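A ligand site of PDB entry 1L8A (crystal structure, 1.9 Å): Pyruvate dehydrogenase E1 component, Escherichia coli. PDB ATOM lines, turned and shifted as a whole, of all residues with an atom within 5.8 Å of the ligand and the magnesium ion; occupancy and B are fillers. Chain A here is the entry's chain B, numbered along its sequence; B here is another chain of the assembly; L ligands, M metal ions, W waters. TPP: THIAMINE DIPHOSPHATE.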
ATOM      1  N   HIS A 106     -29.665 -15.678  23.012  1.00  0.00           N
ATOM      2  CA  HIS A 106     -29.133 -15.514  24.367  1.00  0.00           C
ATOM      3  C   HIS A 106     -28.748 -14.078  24.728  1.00  0.00           C
ATOM      4  O   HIS A 106     -28.405 -13.282  23.846  1.00  0.00           O
ATOM      5  CB  HIS A 106     -27.903 -16.402  24.576  1.00  0.00           C
ATOM      6  CG  HIS A 106     -28.061 -17.791  24.026  1.00  0.00           C
ATOM      7  ND1 HIS A 106     -27.849 -18.920  24.784  1.00  0.00           N
ATOM      8  CD2 HIS A 106     -28.410 -18.221  22.787  1.00  0.00           C
ATOM      9  CE1 HIS A 106     -28.069 -19.986  24.032  1.00  0.00           C
ATOM     10  NE2 HIS A 106     -28.408 -19.590  22.821  1.00  0.00           N
ATOM     11  N   SER A 109     -24.982 -14.448  28.532  1.00  0.00           N
ATOM     12  CA  SER A 109     -23.572 -14.684  28.222  1.00  0.00           C
ATOM     13  C   SER A 109     -22.836 -13.446  27.735  1.00  0.00           C
ATOM     14  O   SER A 109     -21.731 -13.138  28.215  1.00  0.00           O
ATOM     15  CB  SER A 109     -23.430 -15.803  27.203  1.00  0.00           C
ATOM     16  OG  SER A 109     -22.059 -16.055  26.922  1.00  0.00           O
ATOM     17  N   SER A 112     -21.866 -10.947  30.431  1.00  0.00           N
ATOM     18  CA  SER A 112     -20.701 -11.238  31.256  1.00  0.00           C
ATOM     19  C   SER A 112     -19.369 -10.987  30.544  1.00  0.00           C
ATOM     20  O   SER A 112     -18.351 -10.748  31.193  1.00  0.00           O
ATOM     21  CB  SER A 112     -20.746 -12.689  31.744  1.00  0.00           C
ATOM     22  OG  SER A 112     -20.685 -13.604  30.657  1.00  0.00           O
ATOM     23  N   GLN A 140     -17.250 -16.032  20.361  1.00  0.00           N
ATOM     24  CA  GLN A 140     -18.058 -17.066  20.982  1.00  0.00           C
ATOM     25  C   GLN A 140     -19.420 -16.995  20.286  1.00  0.00           C
ATOM     26  O   GLN A 140     -20.012 -15.930  20.157  1.00  0.00           O
ATOM     27  CB  GLN A 140     -18.195 -16.793  22.466  1.00  0.00           C
ATOM     28  CG  GLN A 140     -18.726 -17.946  23.298  1.00  0.00           C
ATOM     29  CD  GLN A 140     -18.870 -17.552  24.751  1.00  0.00           C
ATOM     30  OE1 GLN A 140     -18.930 -16.370  25.077  1.00  0.00           O
ATOM     31  NE2 GLN A 140     -18.918 -18.542  25.638  1.00  0.00           N
ATOM     32  N   HIS A 142     -22.847 -17.812  20.777  1.00  0.00           N
ATOM     33  CA  HIS A 142     -24.065 -17.207  21.320  1.00  0.00           C
ATOM     34  C   HIS A 142     -24.008 -15.777  21.839  1.00  0.00           C
ATOM     35  O   HIS A 142     -24.997 -15.286  22.389  1.00  0.00           O
ATOM     36  CB  HIS A 142     -24.673 -18.131  22.384  1.00  0.00           C
ATOM     37  CG  HIS A 142     -23.756 -18.448  23.516  1.00  0.00           C
ATOM     38  ND1 HIS A 142     -22.707 -19.344  23.405  1.00  0.00           N
ATOM     39  CD2 HIS A 142     -23.737 -18.003  24.791  1.00  0.00           C
ATOM     40  CE1 HIS A 142     -22.076 -19.427  24.559  1.00  0.00           C
ATOM     41  NE2 HIS A 142     -22.679 -18.622  25.415  1.00  0.00           N
ATOM     42  N   VAL A 192     -20.348 -21.943  17.133  1.00  0.00           N
ATOM     43  CA  VAL A 192     -21.414 -22.439  18.025  1.00  0.00           C
ATOM     44  C   VAL A 192     -21.306 -23.887  18.435  1.00  0.00           C
ATOM     45  O   VAL A 192     -21.760 -24.237  19.506  1.00  0.00           O
ATOM     46  CB  VAL A 192     -22.850 -22.292  17.485  1.00  0.00           C
ATOM     47  CG1 VAL A 192     -23.701 -21.611  18.549  1.00  0.00           C
ATOM     48  CG2 VAL A 192     -22.882 -21.579  16.198  1.00  0.00           C
ATOM     49  N   SER A 193     -20.767 -24.742  17.568  1.00  0.00           N
ATOM     50  CA  SER A 193     -20.609 -26.113  17.989  1.00  0.00           C
ATOM     51  C   SER A 193     -19.364 -26.027  18.856  1.00  0.00           C
ATOM     52  O   SER A 193     -18.237 -26.002  18.367  1.00  0.00           O
ATOM     53  CB  SER A 193     -20.367 -27.059  16.813  1.00  0.00           C
ATOM     54  OG  SER A 193     -20.285 -28.399  17.291  1.00  0.00           O
ATOM     55  N   MET A 194     -19.599 -25.955  20.169  1.00  0.00           N
ATOM     56  CA  MET A 194     -18.523 -25.810  21.124  1.00  0.00           C
ATOM     57  C   MET A 194     -17.438 -26.871  21.043  1.00  0.00           C
ATOM     58  O   MET A 194     -17.695 -28.034  20.690  1.00  0.00           O
ATOM     59  CB  MET A 194     -19.113 -25.755  22.538  1.00  0.00           C
ATOM     60  CG  MET A 194     -19.828 -24.441  22.796  1.00  0.00           C
ATOM     61  SD  MET A 194     -20.952 -24.463  24.175  1.00  0.00           S
ATOM     62  CE  MET A 194     -21.685 -22.858  23.995  1.00  0.00           C
ATOM     63  N   GLY A 195     -16.214 -26.451  21.357  1.00  0.00           N
ATOM     64  CA  GLY A 195     -15.069 -27.331  21.314  1.00  0.00           C
ATOM     65  C   GLY A 195     -14.343 -27.235  19.983  1.00  0.00           C
ATOM     66  O   GLY A 195     -13.154 -27.497  19.899  1.00  0.00           O
ATOM     67  N   LEU A 228     -13.654 -18.369  24.241  1.00  0.00           N
ATOM     68  CA  LEU A 228     -14.317 -19.571  24.743  1.00  0.00           C
ATOM     69  C   LEU A 228     -15.113 -19.392  26.036  1.00  0.00           C
ATOM     70  O   LEU A 228     -14.961 -18.408  26.752  1.00  0.00           O
ATOM     71  CB  LEU A 228     -13.267 -20.667  24.959  1.00  0.00           C
ATOM     72  CG  LEU A 228     -12.101 -20.655  23.967  1.00  0.00           C
ATOM     73  CD1 LEU A 228     -10.912 -21.435  24.527  1.00  0.00           C
ATOM     74  CD2 LEU A 228     -12.557 -21.259  22.648  1.00  0.00           C
ATOM     75  N   GLY A 229     -15.957 -20.386  26.319  1.00  0.00           N
ATOM     76  CA  GLY A 229     -16.739 -20.376  27.526  1.00  0.00           C
ATOM     77  C   GLY A 229     -15.998 -21.326  28.445  1.00  0.00           C
ATOM     78  O   GLY A 229     -15.239 -22.166  27.958  1.00  0.00           O
ATOM     79  N   ASP A 230     -16.166 -21.194  29.769  1.00  0.00           N
ATOM     80  CA  ASP A 230     -15.437 -22.129  30.617  1.00  0.00           C
ATOM     81  C   ASP A 230     -16.101 -23.502  30.573  1.00  0.00           C
ATOM     82  O   ASP A 230     -15.433 -24.512  30.649  1.00  0.00           O
ATOM     83  CB  ASP A 230     -15.299 -21.611  32.062  1.00  0.00           C
ATOM     84  CG  ASP A 230     -16.601 -21.123  32.649  1.00  0.00           C
ATOM     85  OD1 ASP A 230     -17.630 -21.196  31.969  1.00  0.00           O
ATOM     86  OD2 ASP A 230     -16.600 -20.674  33.809  1.00  0.00           O
ATOM     87  N   GLY A 231     -17.431 -23.531  30.435  1.00  0.00           N
ATOM     88  CA  GLY A 231     -18.124 -24.806  30.379  1.00  0.00           C
ATOM     89  C   GLY A 231     -17.683 -25.563  29.136  1.00  0.00           C
ATOM     90  O   GLY A 231     -17.483 -26.774  29.166  1.00  0.00           O
ATOM     91  N   GLU A 232     -17.536 -24.810  28.038  1.00  0.00           N
ATOM     92  CA  GLU A 232     -17.118 -25.354  26.757  1.00  0.00           C
ATOM     93  C   GLU A 232     -15.757 -26.071  26.839  1.00  0.00           C
ATOM     94  O   GLU A 232     -15.474 -26.984  26.059  1.00  0.00           O
ATOM     95  CB  GLU A 232     -17.036 -24.208  25.734  1.00  0.00           C
ATOM     96  CG  GLU A 232     -16.182 -24.527  24.510  1.00  0.00           C
ATOM     97  CD  GLU A 232     -16.215 -23.432  23.456  1.00  0.00           C
ATOM     98  OE1 GLU A 232     -16.486 -22.262  23.810  1.00  0.00           O
ATOM     99  OE2 GLU A 232     -15.956 -23.760  22.276  1.00  0.00           O
ATOM    100  N   MET A 233     -14.921 -25.669  27.796  1.00  0.00           N
ATOM    101  CA  MET A 233     -13.609 -26.300  27.943  1.00  0.00           C
ATOM    102  C   MET A 233     -13.698 -27.788  28.321  1.00  0.00           C
ATOM    103  O   MET A 233     -12.694 -28.503  28.302  1.00  0.00           O
ATOM    104  CB  MET A 233     -12.772 -25.530  28.981  1.00  0.00           C
ATOM    105  CG  MET A 233     -12.489 -24.065  28.613  1.00  0.00           C
ATOM    106  SD  MET A 233     -12.025 -23.795  26.869  1.00  0.00           S
ATOM    107  CE  MET A 233     -10.355 -24.454  26.870  1.00  0.00           C
ATOM    108  N   GLU A 235     -15.356 -29.932  26.587  1.00  0.00           N
ATOM    109  CA  GLU A 235     -15.346 -30.678  25.319  1.00  0.00           C
ATOM    110  C   GLU A 235     -13.907 -31.161  25.142  1.00  0.00           C
ATOM    111  O   GLU A 235     -12.968 -30.372  25.263  1.00  0.00           O
ATOM    112  CB  GLU A 235     -15.724 -29.759  24.137  1.00  0.00           C
ATOM    113  CG  GLU A 235     -17.165 -29.247  24.103  1.00  0.00           C
ATOM    114  CD  GLU A 235     -18.176 -30.334  23.779  1.00  0.00           C
ATOM    115  OE1 GLU A 235     -19.361 -29.992  23.546  1.00  0.00           O
ATOM    116  OE2 GLU A 235     -17.806 -31.527  23.770  1.00  0.00           O
ATOM    117  N   ASN A 258     -13.986 -17.155  29.092  1.00  0.00           N
ATOM    118  CA  ASN A 258     -14.901 -16.418  29.948  1.00  0.00           C
ATOM    119  C   ASN A 258     -15.181 -17.299  31.159  1.00  0.00           C
ATOM    120  O   ASN A 258     -15.891 -18.288  31.064  1.00  0.00           O
ATOM    121  CB  ASN A 258     -16.205 -16.101  29.223  1.00  0.00           C
ATOM    122  CG  ASN A 258     -17.109 -15.198  30.026  1.00  0.00           C
ATOM    123  OD1 ASN A 258     -16.763 -14.812  31.143  1.00  0.00           O
ATOM    124  ND2 ASN A 258     -18.251 -14.846  29.463  1.00  0.00           N
ATOM    125  N   CYS A 259     -14.600 -16.942  32.298  1.00  0.00           N
ATOM    126  CA  CYS A 259     -14.774 -17.737  33.504  1.00  0.00           C
ATOM    127  C   CYS A 259     -15.838 -17.176  34.438  1.00  0.00           C
ATOM    128  O   CYS A 259     -15.524 -16.595  35.473  1.00  0.00           O
ATOM    129  CB  CYS A 259     -13.439 -17.872  34.237  1.00  0.00           C
ATOM    130  SG  CYS A 259     -12.145 -18.783  33.287  1.00  0.00           S
ATOM    131  N   ASN A 260     -17.107 -17.363  34.056  1.00  0.00           N
ATOM    132  CA  ASN A 260     -18.222 -16.903  34.871  1.00  0.00           C
ATOM    133  C   ASN A 260     -18.635 -18.037  35.806  1.00  0.00           C
ATOM    134  O   ASN A 260     -19.634 -17.927  36.517  1.00  0.00           O
ATOM    135  CB  ASN A 260     -19.406 -16.453  34.007  1.00  0.00           C
ATOM    136  CG  ASN A 260     -19.708 -17.428  32.891  1.00  0.00           C
ATOM    137  OD1 ASN A 260     -19.516 -18.623  33.042  1.00  0.00           O
ATOM    138  ND2 ASN A 260     -20.191 -16.908  31.767  1.00  0.00           N
ATOM    139  N   LEU A 261     -17.853 -19.126  35.796  1.00  0.00           N
ATOM    140  CA  LEU A 261     -18.043 -20.308  36.640  1.00  0.00           C
ATOM    141  C   LEU A 261     -19.277 -21.164  36.362  1.00  0.00           C
ATOM    142  O   LEU A 261     -19.527 -22.152  37.057  1.00  0.00           O
ATOM    143  CB  LEU A 261     -18.046 -19.916  38.123  1.00  0.00           C
ATOM    144  CG  LEU A 261     -17.090 -18.815  38.614  1.00  0.00           C
ATOM    145  CD1 LEU A 261     -17.316 -18.560  40.107  1.00  0.00           C
ATOM    146  CD2 LEU A 261     -15.650 -19.213  38.362  1.00  0.00           C
ATOM    147  N   GLN A 262     -20.020 -20.808  35.330  1.00  0.00           N
ATOM    148  CA  GLN A 262     -21.245 -21.518  35.030  1.00  0.00           C
ATOM    149  C   GLN A 262     -21.420 -21.924  33.569  1.00  0.00           C
ATOM    150  O   GLN A 262     -21.027 -21.192  32.671  1.00  0.00           O
ATOM    151  CB  GLN A 262     -22.431 -20.627  35.429  1.00  0.00           C
ATOM    152  CG  GLN A 262     -23.697 -21.373  35.828  1.00  0.00           C
ATOM    153  CD  GLN A 262     -23.859 -21.500  37.339  1.00  0.00           C
ATOM    154  OE1 GLN A 262     -24.895 -21.938  37.828  1.00  0.00           O
ATOM    155  NE2 GLN A 262     -22.827 -21.104  38.091  1.00  0.00           N
ATOM    156  N   ARG A 263     -21.998 -23.108  33.333  1.00  0.00           N
ATOM    157  CA  ARG A 263     -22.281 -23.502  31.953  1.00  0.00           C
ATOM    158  C   ARG A 263     -23.755 -23.108  31.800  1.00  0.00           C
ATOM    159  O   ARG A 263     -24.288 -22.406  32.657  1.00  0.00           O
ATOM    160  CB  ARG A 263     -22.080 -25.008  31.731  1.00  0.00           C
ATOM    161  CG  ARG A 263     -22.119 -25.856  32.972  1.00  0.00           C
ATOM    162  CD  ARG A 263     -22.462 -27.286  32.636  1.00  0.00           C
ATOM    163  NE  ARG A 263     -23.293 -27.863  33.688  1.00  0.00           N
ATOM    164  CZ  ARG A 263     -22.868 -28.795  34.523  1.00  0.00           C
ATOM    165  NH1 ARG A 263     -21.628 -29.251  34.409  1.00  0.00           N
ATOM    166  NH2 ARG A 263     -23.659 -29.249  35.475  1.00  0.00           N
ATOM    167  N   LEU A 264     -24.423 -23.547  30.736  1.00  0.00           N
ATOM    168  CA  LEU A 264     -25.965 -23.562  30.894  1.00  0.00           C
ATOM    169  C   LEU A 264     -26.866 -23.838  32.098  1.00  0.00           C
ATOM    170  O   LEU A 264     -27.495 -22.920  32.646  1.00  0.00           O
ATOM    171  CB  LEU A 264     -26.516 -24.319  29.686  1.00  0.00           C
ATOM    172  CG  LEU A 264     -27.424 -23.606  28.671  1.00  0.00           C
ATOM    173  CD1 LEU A 264     -28.744 -24.350  28.585  1.00  0.00           C
ATOM    174  CD2 LEU A 264     -27.650 -22.162  29.077  1.00  0.00           C
ATOM    175  N   VAL A 268     -19.801 -25.029  36.259  1.00  0.00           N
ATOM    176  CA  VAL A 268     -18.977 -26.038  35.603  1.00  0.00           C
ATOM    177  C   VAL A 268     -18.507 -27.050  36.651  1.00  0.00           C
ATOM    178  O   VAL A 268     -18.624 -28.267  36.444  1.00  0.00           O
ATOM    179  CB  VAL A 268     -17.736 -25.415  34.918  1.00  0.00           C
ATOM    180  CG1 VAL A 268     -16.963 -26.481  34.152  1.00  0.00           C
ATOM    181  CG2 VAL A 268     -18.168 -24.298  33.985  1.00  0.00           C
ATOM    182  N   LYS A 392     -22.094 -14.097  35.146  1.00  0.00           N
ATOM    183  CA  LYS A 392     -22.955 -14.470  34.024  1.00  0.00           C
ATOM    184  C   LYS A 392     -24.178 -13.575  33.802  1.00  0.00           C
ATOM    185  O   LYS A 392     -24.286 -12.923  32.760  1.00  0.00           O
ATOM    186  CB  LYS A 392     -23.400 -15.928  34.135  1.00  0.00           C
ATOM    187  CG  LYS A 392     -24.264 -16.409  32.960  1.00  0.00           C
ATOM    188  CD  LYS A 392     -23.499 -17.356  32.038  1.00  0.00           C
ATOM    189  CE  LYS A 392     -24.066 -18.776  32.106  1.00  0.00           C
ATOM    190  NZ  LYS A 392     -24.053 -19.460  30.779  1.00  0.00           N
ATOM    191  N   ASP A 609     -18.215 -33.355  12.648  1.00  0.00           N
ATOM    192  CA  ASP A 609     -18.735 -32.052  13.053  1.00  0.00           C
ATOM    193  C   ASP A 609     -17.859 -30.958  12.466  1.00  0.00           C
ATOM    194  O   ASP A 609     -18.354 -29.893  12.104  1.00  0.00           O
ATOM    195  CB  ASP A 609     -18.782 -31.933  14.587  1.00  0.00           C
ATOM    196  CG  ASP A 609     -19.912 -31.019  15.086  1.00  0.00           C
ATOM    197  OD1 ASP A 609     -20.884 -30.760  14.337  1.00  0.00           O
ATOM    198  OD2 ASP A 609     -19.822 -30.551  16.237  1.00  0.00           O
ATOM    199  N   ALA B 520     -25.881 -33.791  28.740  1.00  0.00           N
ATOM    200  CA  ALA B 520     -24.632 -33.078  28.480  1.00  0.00           C
ATOM    201  C   ALA B 520     -24.964 -31.605  28.752  1.00  0.00           C
ATOM    202  O   ALA B 520     -25.239 -30.841  27.830  1.00  0.00           O
ATOM    203  CB  ALA B 520     -24.186 -33.281  27.032  1.00  0.00           C
ATOM    204  N   ASP B 521     -24.947 -31.246  30.023  1.00  0.00           N
ATOM    205  CA  ASP B 521     -25.260 -29.906  30.500  1.00  0.00           C
ATOM    206  C   ASP B 521     -26.757 -29.597  30.491  1.00  0.00           C
ATOM    207  O   ASP B 521     -27.401 -29.527  31.536  1.00  0.00           O
ATOM    208  CB  ASP B 521     -24.524 -28.824  29.708  1.00  0.00           C
ATOM    209  CG  ASP B 521     -24.754 -27.419  30.280  1.00  0.00           C
ATOM    210  OD1 ASP B 521     -25.327 -27.301  31.389  1.00  0.00           O
ATOM    211  OD2 ASP B 521     -24.359 -26.424  29.637  1.00  0.00           O
ATOM    212  N   GLU B 522     -27.316 -29.425  29.294  1.00  0.00           N
ATOM    213  CA  GLU B 522     -28.719 -29.070  29.142  1.00  0.00           C
ATOM    214  C   GLU B 522     -29.771 -30.141  29.460  1.00  0.00           C
ATOM    215  O   GLU B 522     -29.837 -31.181  28.803  1.00  0.00           O
ATOM    216  CB  GLU B 522     -28.958 -28.501  27.752  1.00  0.00           C
ATOM    217  CG  GLU B 522     -28.031 -27.337  27.448  1.00  0.00           C
ATOM    218  CD  GLU B 522     -28.467 -26.535  26.251  1.00  0.00           C
ATOM    219  OE1 GLU B 522     -27.617 -25.797  25.700  1.00  0.00           O
ATOM    220  OE2 GLU B 522     -29.639 -26.632  25.846  1.00  0.00           O
ATOM    221  N   ILE B 569     -20.831 -29.894  29.117  1.00  0.00           N
ATOM    222  CA  ILE B 569     -20.637 -29.693  27.672  1.00  0.00           C
ATOM    223  C   ILE B 569     -19.546 -30.645  27.197  1.00  0.00           C
ATOM    224  O   ILE B 569     -18.397 -30.247  26.985  1.00  0.00           O
ATOM    225  CB  ILE B 569     -20.245 -28.228  27.384  1.00  0.00           C
ATOM    226  CG1 ILE B 569     -21.107 -27.298  28.238  1.00  0.00           C
ATOM    227  CG2 ILE B 569     -20.430 -27.920  25.893  1.00  0.00           C
ATOM    228  CD1 ILE B 569     -20.912 -25.818  27.941  1.00  0.00           C
ATOM    229  N   GLU B 571     -20.150 -34.019  24.784  1.00  0.00           N
ATOM    230  CA  GLU B 571     -20.923 -35.078  24.136  1.00  0.00           C
ATOM    231  C   GLU B 571     -20.163 -36.385  24.073  1.00  0.00           C
ATOM    232  O   GLU B 571     -20.739 -37.455  24.259  1.00  0.00           O
ATOM    233  CB  GLU B 571     -21.345 -34.640  22.736  1.00  0.00           C
ATOM    234  CG  GLU B 571     -22.559 -33.734  22.729  1.00  0.00           C
ATOM    235  CD  GLU B 571     -22.214 -32.274  22.944  1.00  0.00           C
ATOM    236  OE1 GLU B 571     -21.018 -31.924  22.927  1.00  0.00           O
ATOM    237  OE2 GLU B 571     -23.141 -31.468  23.134  1.00  0.00           O
ATOM    238  N   TYR B 599     -28.597 -32.674  21.861  1.00  0.00           N
ATOM    239  CA  TYR B 599     -28.976 -32.080  20.572  1.00  0.00           C
ATOM    240  C   TYR B 599     -28.596 -33.102  19.492  1.00  0.00           C
ATOM    241  O   TYR B 599     -27.418 -33.404  19.314  1.00  0.00           O
ATOM    242  CB  TYR B 599     -28.179 -30.810  20.310  1.00  0.00           C
ATOM    243  CG  TYR B 599     -28.663 -29.601  21.067  1.00  0.00           C
ATOM    244  CD1 TYR B 599     -28.215 -29.339  22.359  1.00  0.00           C
ATOM    245  CD2 TYR B 599     -29.581 -28.725  20.500  1.00  0.00           C
ATOM    246  CE1 TYR B 599     -28.669 -28.230  23.070  1.00  0.00           C
ATOM    247  CE2 TYR B 599     -30.036 -27.616  21.189  1.00  0.00           C
ATOM    248  CZ  TYR B 599     -29.579 -27.379  22.472  1.00  0.00           C
ATOM    249  OH  TYR B 599     -30.042 -26.278  23.152  1.00  0.00           O
ATOM    250  N   PHE B 602     -25.321 -33.046  17.494  1.00  0.00           N
ATOM    251  CA  PHE B 602     -24.068 -33.354  18.167  1.00  0.00           C
ATOM    252  C   PHE B 602     -23.952 -34.838  18.554  1.00  0.00           C
ATOM    253  O   PHE B 602     -23.230 -35.209  19.479  1.00  0.00           O
ATOM    254  CB  PHE B 602     -23.914 -32.448  19.393  1.00  0.00           C
ATOM    255  CG  PHE B 602     -24.063 -30.982  19.088  1.00  0.00           C
ATOM    256  CD1 PHE B 602     -24.832 -30.154  19.898  1.00  0.00           C
ATOM    257  CD2 PHE B 602     -23.468 -30.419  17.962  1.00  0.00           C
ATOM    258  CE1 PHE B 602     -25.018 -28.802  19.590  1.00  0.00           C
ATOM    259  CE2 PHE B 602     -23.636 -29.086  17.653  1.00  0.00           C
ATOM    260  CZ  PHE B 602     -24.410 -28.267  18.463  1.00  0.00           C
ATOM    261  N   ARG B 606     -20.897 -35.658  15.611  1.00  0.00           N
ATOM    262  CA  ARG B 606     -19.842 -35.258  16.522  1.00  0.00           C
ATOM    263  C   ARG B 606     -19.100 -36.417  17.195  1.00  0.00           C
ATOM    264  O   ARG B 606     -17.883 -36.352  17.410  1.00  0.00           O
ATOM    265  CB  ARG B 606     -20.428 -34.327  17.588  1.00  0.00           C
ATOM    266  CG  ARG B 606     -19.431 -33.783  18.615  1.00  0.00           C
ATOM    267  CD  ARG B 606     -18.357 -32.888  17.978  1.00  0.00           C
ATOM    268  NE  ARG B 606     -17.519 -32.259  18.989  1.00  0.00           N
ATOM    269  CZ  ARG B 606     -17.667 -31.007  19.431  1.00  0.00           C
ATOM    270  NH1 ARG B 606     -18.619 -30.246  18.929  1.00  0.00           N
ATOM    271  NH2 ARG B 606     -16.874 -30.545  20.377  1.00  0.00           N
ATOM    272  N   HIS B 640     -26.967 -26.463  14.022  1.00  0.00           N
ATOM    273  CA  HIS B 640     -27.890 -27.101  14.962  1.00  0.00           C
ATOM    274  C   HIS B 640     -29.006 -27.894  14.280  1.00  0.00           C
ATOM    275  O   HIS B 640     -29.389 -28.961  14.744  1.00  0.00           O
ATOM    276  CB  HIS B 640     -28.550 -26.058  15.848  1.00  0.00           C
ATOM    277  CG  HIS B 640     -27.659 -25.535  16.937  1.00  0.00           C
ATOM    278  ND1 HIS B 640     -26.709 -24.562  16.722  1.00  0.00           N
ATOM    279  CD2 HIS B 640     -27.614 -25.822  18.264  1.00  0.00           C
ATOM    280  CE1 HIS B 640     -26.122 -24.261  17.869  1.00  0.00           C
ATOM    281  NE2 HIS B 640     -26.652 -25.003  18.813  1.00  0.00           N
HETATM  282  N1' TPP L   1     -23.055 -28.719  22.691  1.00  0.00           N
HETATM  283  C2' TPP L   1     -22.292 -28.136  21.709  1.00  0.00           C
HETATM  284  CM2 TPP L   1     -21.253 -28.984  21.053  1.00  0.00           C
HETATM  285  N3' TPP L   1     -22.465 -26.866  21.311  1.00  0.00           N
HETATM  286  C4' TPP L   1     -23.462 -26.101  21.907  1.00  0.00           C
HETATM  287  N4' TPP L   1     -23.596 -24.870  21.458  1.00  0.00           N
HETATM  288  C5' TPP L   1     -24.312 -26.703  22.964  1.00  0.00           C
HETATM  289  C6' TPP L   1     -24.062 -28.004  23.305  1.00  0.00           C
HETATM  290  C7' TPP L   1     -25.476 -25.988  23.626  1.00  0.00           C
HETATM  291  N3  TPP L   1     -25.073 -24.831  24.518  1.00  0.00           N
HETATM  292  C2  TPP L   1     -25.333 -23.569  24.209  1.00  0.00           C
HETATM  293  S1  TPP L   1     -24.855 -22.502  25.412  1.00  0.00           S
HETATM  294  C5  TPP L   1     -24.258 -23.792  26.386  1.00  0.00           C
HETATM  295  C4  TPP L   1     -24.454 -25.005  25.776  1.00  0.00           C
HETATM  296  CM4 TPP L   1     -24.119 -26.369  26.323  1.00  0.00           C
HETATM  297  C6  TPP L   1     -23.525 -23.526  27.657  1.00  0.00           C
HETATM  298  C7  TPP L   1     -22.396 -22.560  27.416  1.00  0.00           C
HETATM  299  O7  TPP L   1     -21.601 -22.504  28.603  1.00  0.00           O
HETATM  300  PA  TPP L   1     -20.117 -21.892  28.578  1.00  0.00           P
HETATM  301  O1A TPP L   1     -19.326 -22.539  27.494  1.00  0.00           O
HETATM  302  O2A TPP L   1     -19.607 -21.966  29.956  1.00  0.00           O
HETATM  303  O3A TPP L   1     -20.343 -20.343  28.169  1.00  0.00           O
HETATM  304  PB  TPP L   1     -21.122 -19.073  28.783  1.00  0.00           P
HETATM  305  O1B TPP L   1     -22.407 -18.947  28.057  1.00  0.00           O
HETATM  306  O2B TPP L   1     -20.226 -17.842  28.486  1.00  0.00           O
HETATM  307  O3B TPP L   1     -21.217 -19.269  30.247  1.00  0.00           O
HETATM  308 MG    MG M   1     -19.406 -20.210  31.629  1.00  0.00          MG
HETATM  309  O   HOH W   1     -19.034 -21.274  25.048  1.00  0.00           O
HETATM  310  O   HOH W   2     -23.571 -29.951  25.649  1.00  0.00           O
HETATM  311  O   HOH W   3     -26.071 -23.190  21.351  1.00  0.00           O
HETATM  312  O   HOH W   4     -18.124 -18.980  30.159  1.00  0.00           O
HETATM  313  O   HOH W   5     -19.620 -15.004  27.138  1.00  0.00           O
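The magnesium ion is bound by the side-chain carboxylate of Asp 230, the side-chain amide oxygen of Asn 260, the backbone carbonyl oxygen of Gln 262, water W4, an oxygen (O2A) of the ligand and an oxygen (O3B) of the ligand. The magnesium ion has six donor atoms within binding distance.
Water W4 lies within hydrogen-bond range of O of Asn 258, O2B of the ligand, N of Asp 230 and ND2 of Asn 260. Water W1 lies within hydrogen-bond range of O1A of the ligand (2.8 Å), NE2 of Gln 140 (2.8 Å), OE1 of Glu 232 (3.0 Å) and N of Gly 229 (3.4 Å). Water W3 bridges a nitrogen (N4') of the ligand and a ring nitrogen (NE2) of His 640 of chain B. Water W5 lies within hydrogen-bond range of OE1 of Gln 140 (2.6 Å), OG of Ser 109 (2.7 Å), ND2 of Asn 258 (2.7 Å) and O2B of the ligand (3.2 Å).
O of Asn 258 sits at hydrogen-bond distance from N of Asp 230, at 3.2 Å. The side-chain carboxylate (OE1) of Glu 571 of chain B lies close to the side-chain carboxylate (OE1) of Glu 235, at 2.6 Å. OE1 of Glu 232 sits at hydrogen-bond distance from N of Gly 229 (3.2 Å). The side-chain carboxylate (OE2) of Glu 232 is in hydrogen-bond range of the backbone NH (N) of Gly 195 (2.9 Å). The backbone carbonyl oxygen (O) of Ser 109 sits at hydrogen-bond distance from the side-chain hydroxyl (OG) of Ser 112 (2.7 Å). The guanidinium group of Arg 606 of chain B lies within hydrogen-bond range of the backbone carbonyl oxygen of Met 194, at 2.7 Å. The backbone NH (N) of Asn 258 lies within hydrogen-bond range of the backbone carbonyl oxygen (O) of Leu 228, 2.8 Å away. The side-chain hydroxyl of Ser 193 lies within hydrogen-bond range of the side-chain carboxylate of Asp 609 (2.4 Å).
Three residues have an atom within 4 Å of the magnesium ion: Asp 230, Asn 260 and Gln 262.
OE1 of Glu 522 of chain B sits close to N3 of the ligand (3.0 Å). Residues that only touch the ligand: Leu 264 (3.2 Å), Glu 235 (3.3 Å), Asp 521 of chain B (3.3 Å), Gly 229 (3.4 Å), Ile 569 of chain B (3.4 Å), Phe 602 of chain B (3.5 Å), Arg 263 (3.6 Å), Arg 606 of chain B (3.6 Å), Asn 258 (3.7 Å), Ser 193 (3.9 Å) and Tyr 599 of chain B (3.9 Å). The nearest printed residue that does not touch the ligand is His 640 of chain B (4.04 Å).
NE2 of His 142 sits at hydrogen-bond distance from O1B of the ligand (2.7 Å). The backbone NH of Gly 231 lies close to an oxygen (O2A) of the ligand (2.7 Å). A nitrogen (N4') of the ligand sits at hydrogen-bond distance from the backbone carbonyl oxygen of Val 192 (2.8 Å). The side-chain carboxylate of Glu 571 of chain B sits at hydrogen-bond distance from a nitrogen (N1') of the ligand, at 2.8 Å. The side-chain amino group (NZ) of Lys 392 is in salt-bridge range of an oxygen (O1B) of the ligand (3.2 Å). The backbone NH of Glu 232 lies within hydrogen-bond range of an oxygen (O1A) of the ligand (2.9 Å). OG of Ser 109 lies within hydrogen-bond range of O2B of the ligand (3.0 Å). NE2 of Gln 140 is in hydrogen-bond range of O2B of the ligand, 3.2 Å away. N3' of the ligand is in hydrogen-bond range of N of Met 194, at 3.2 Å.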
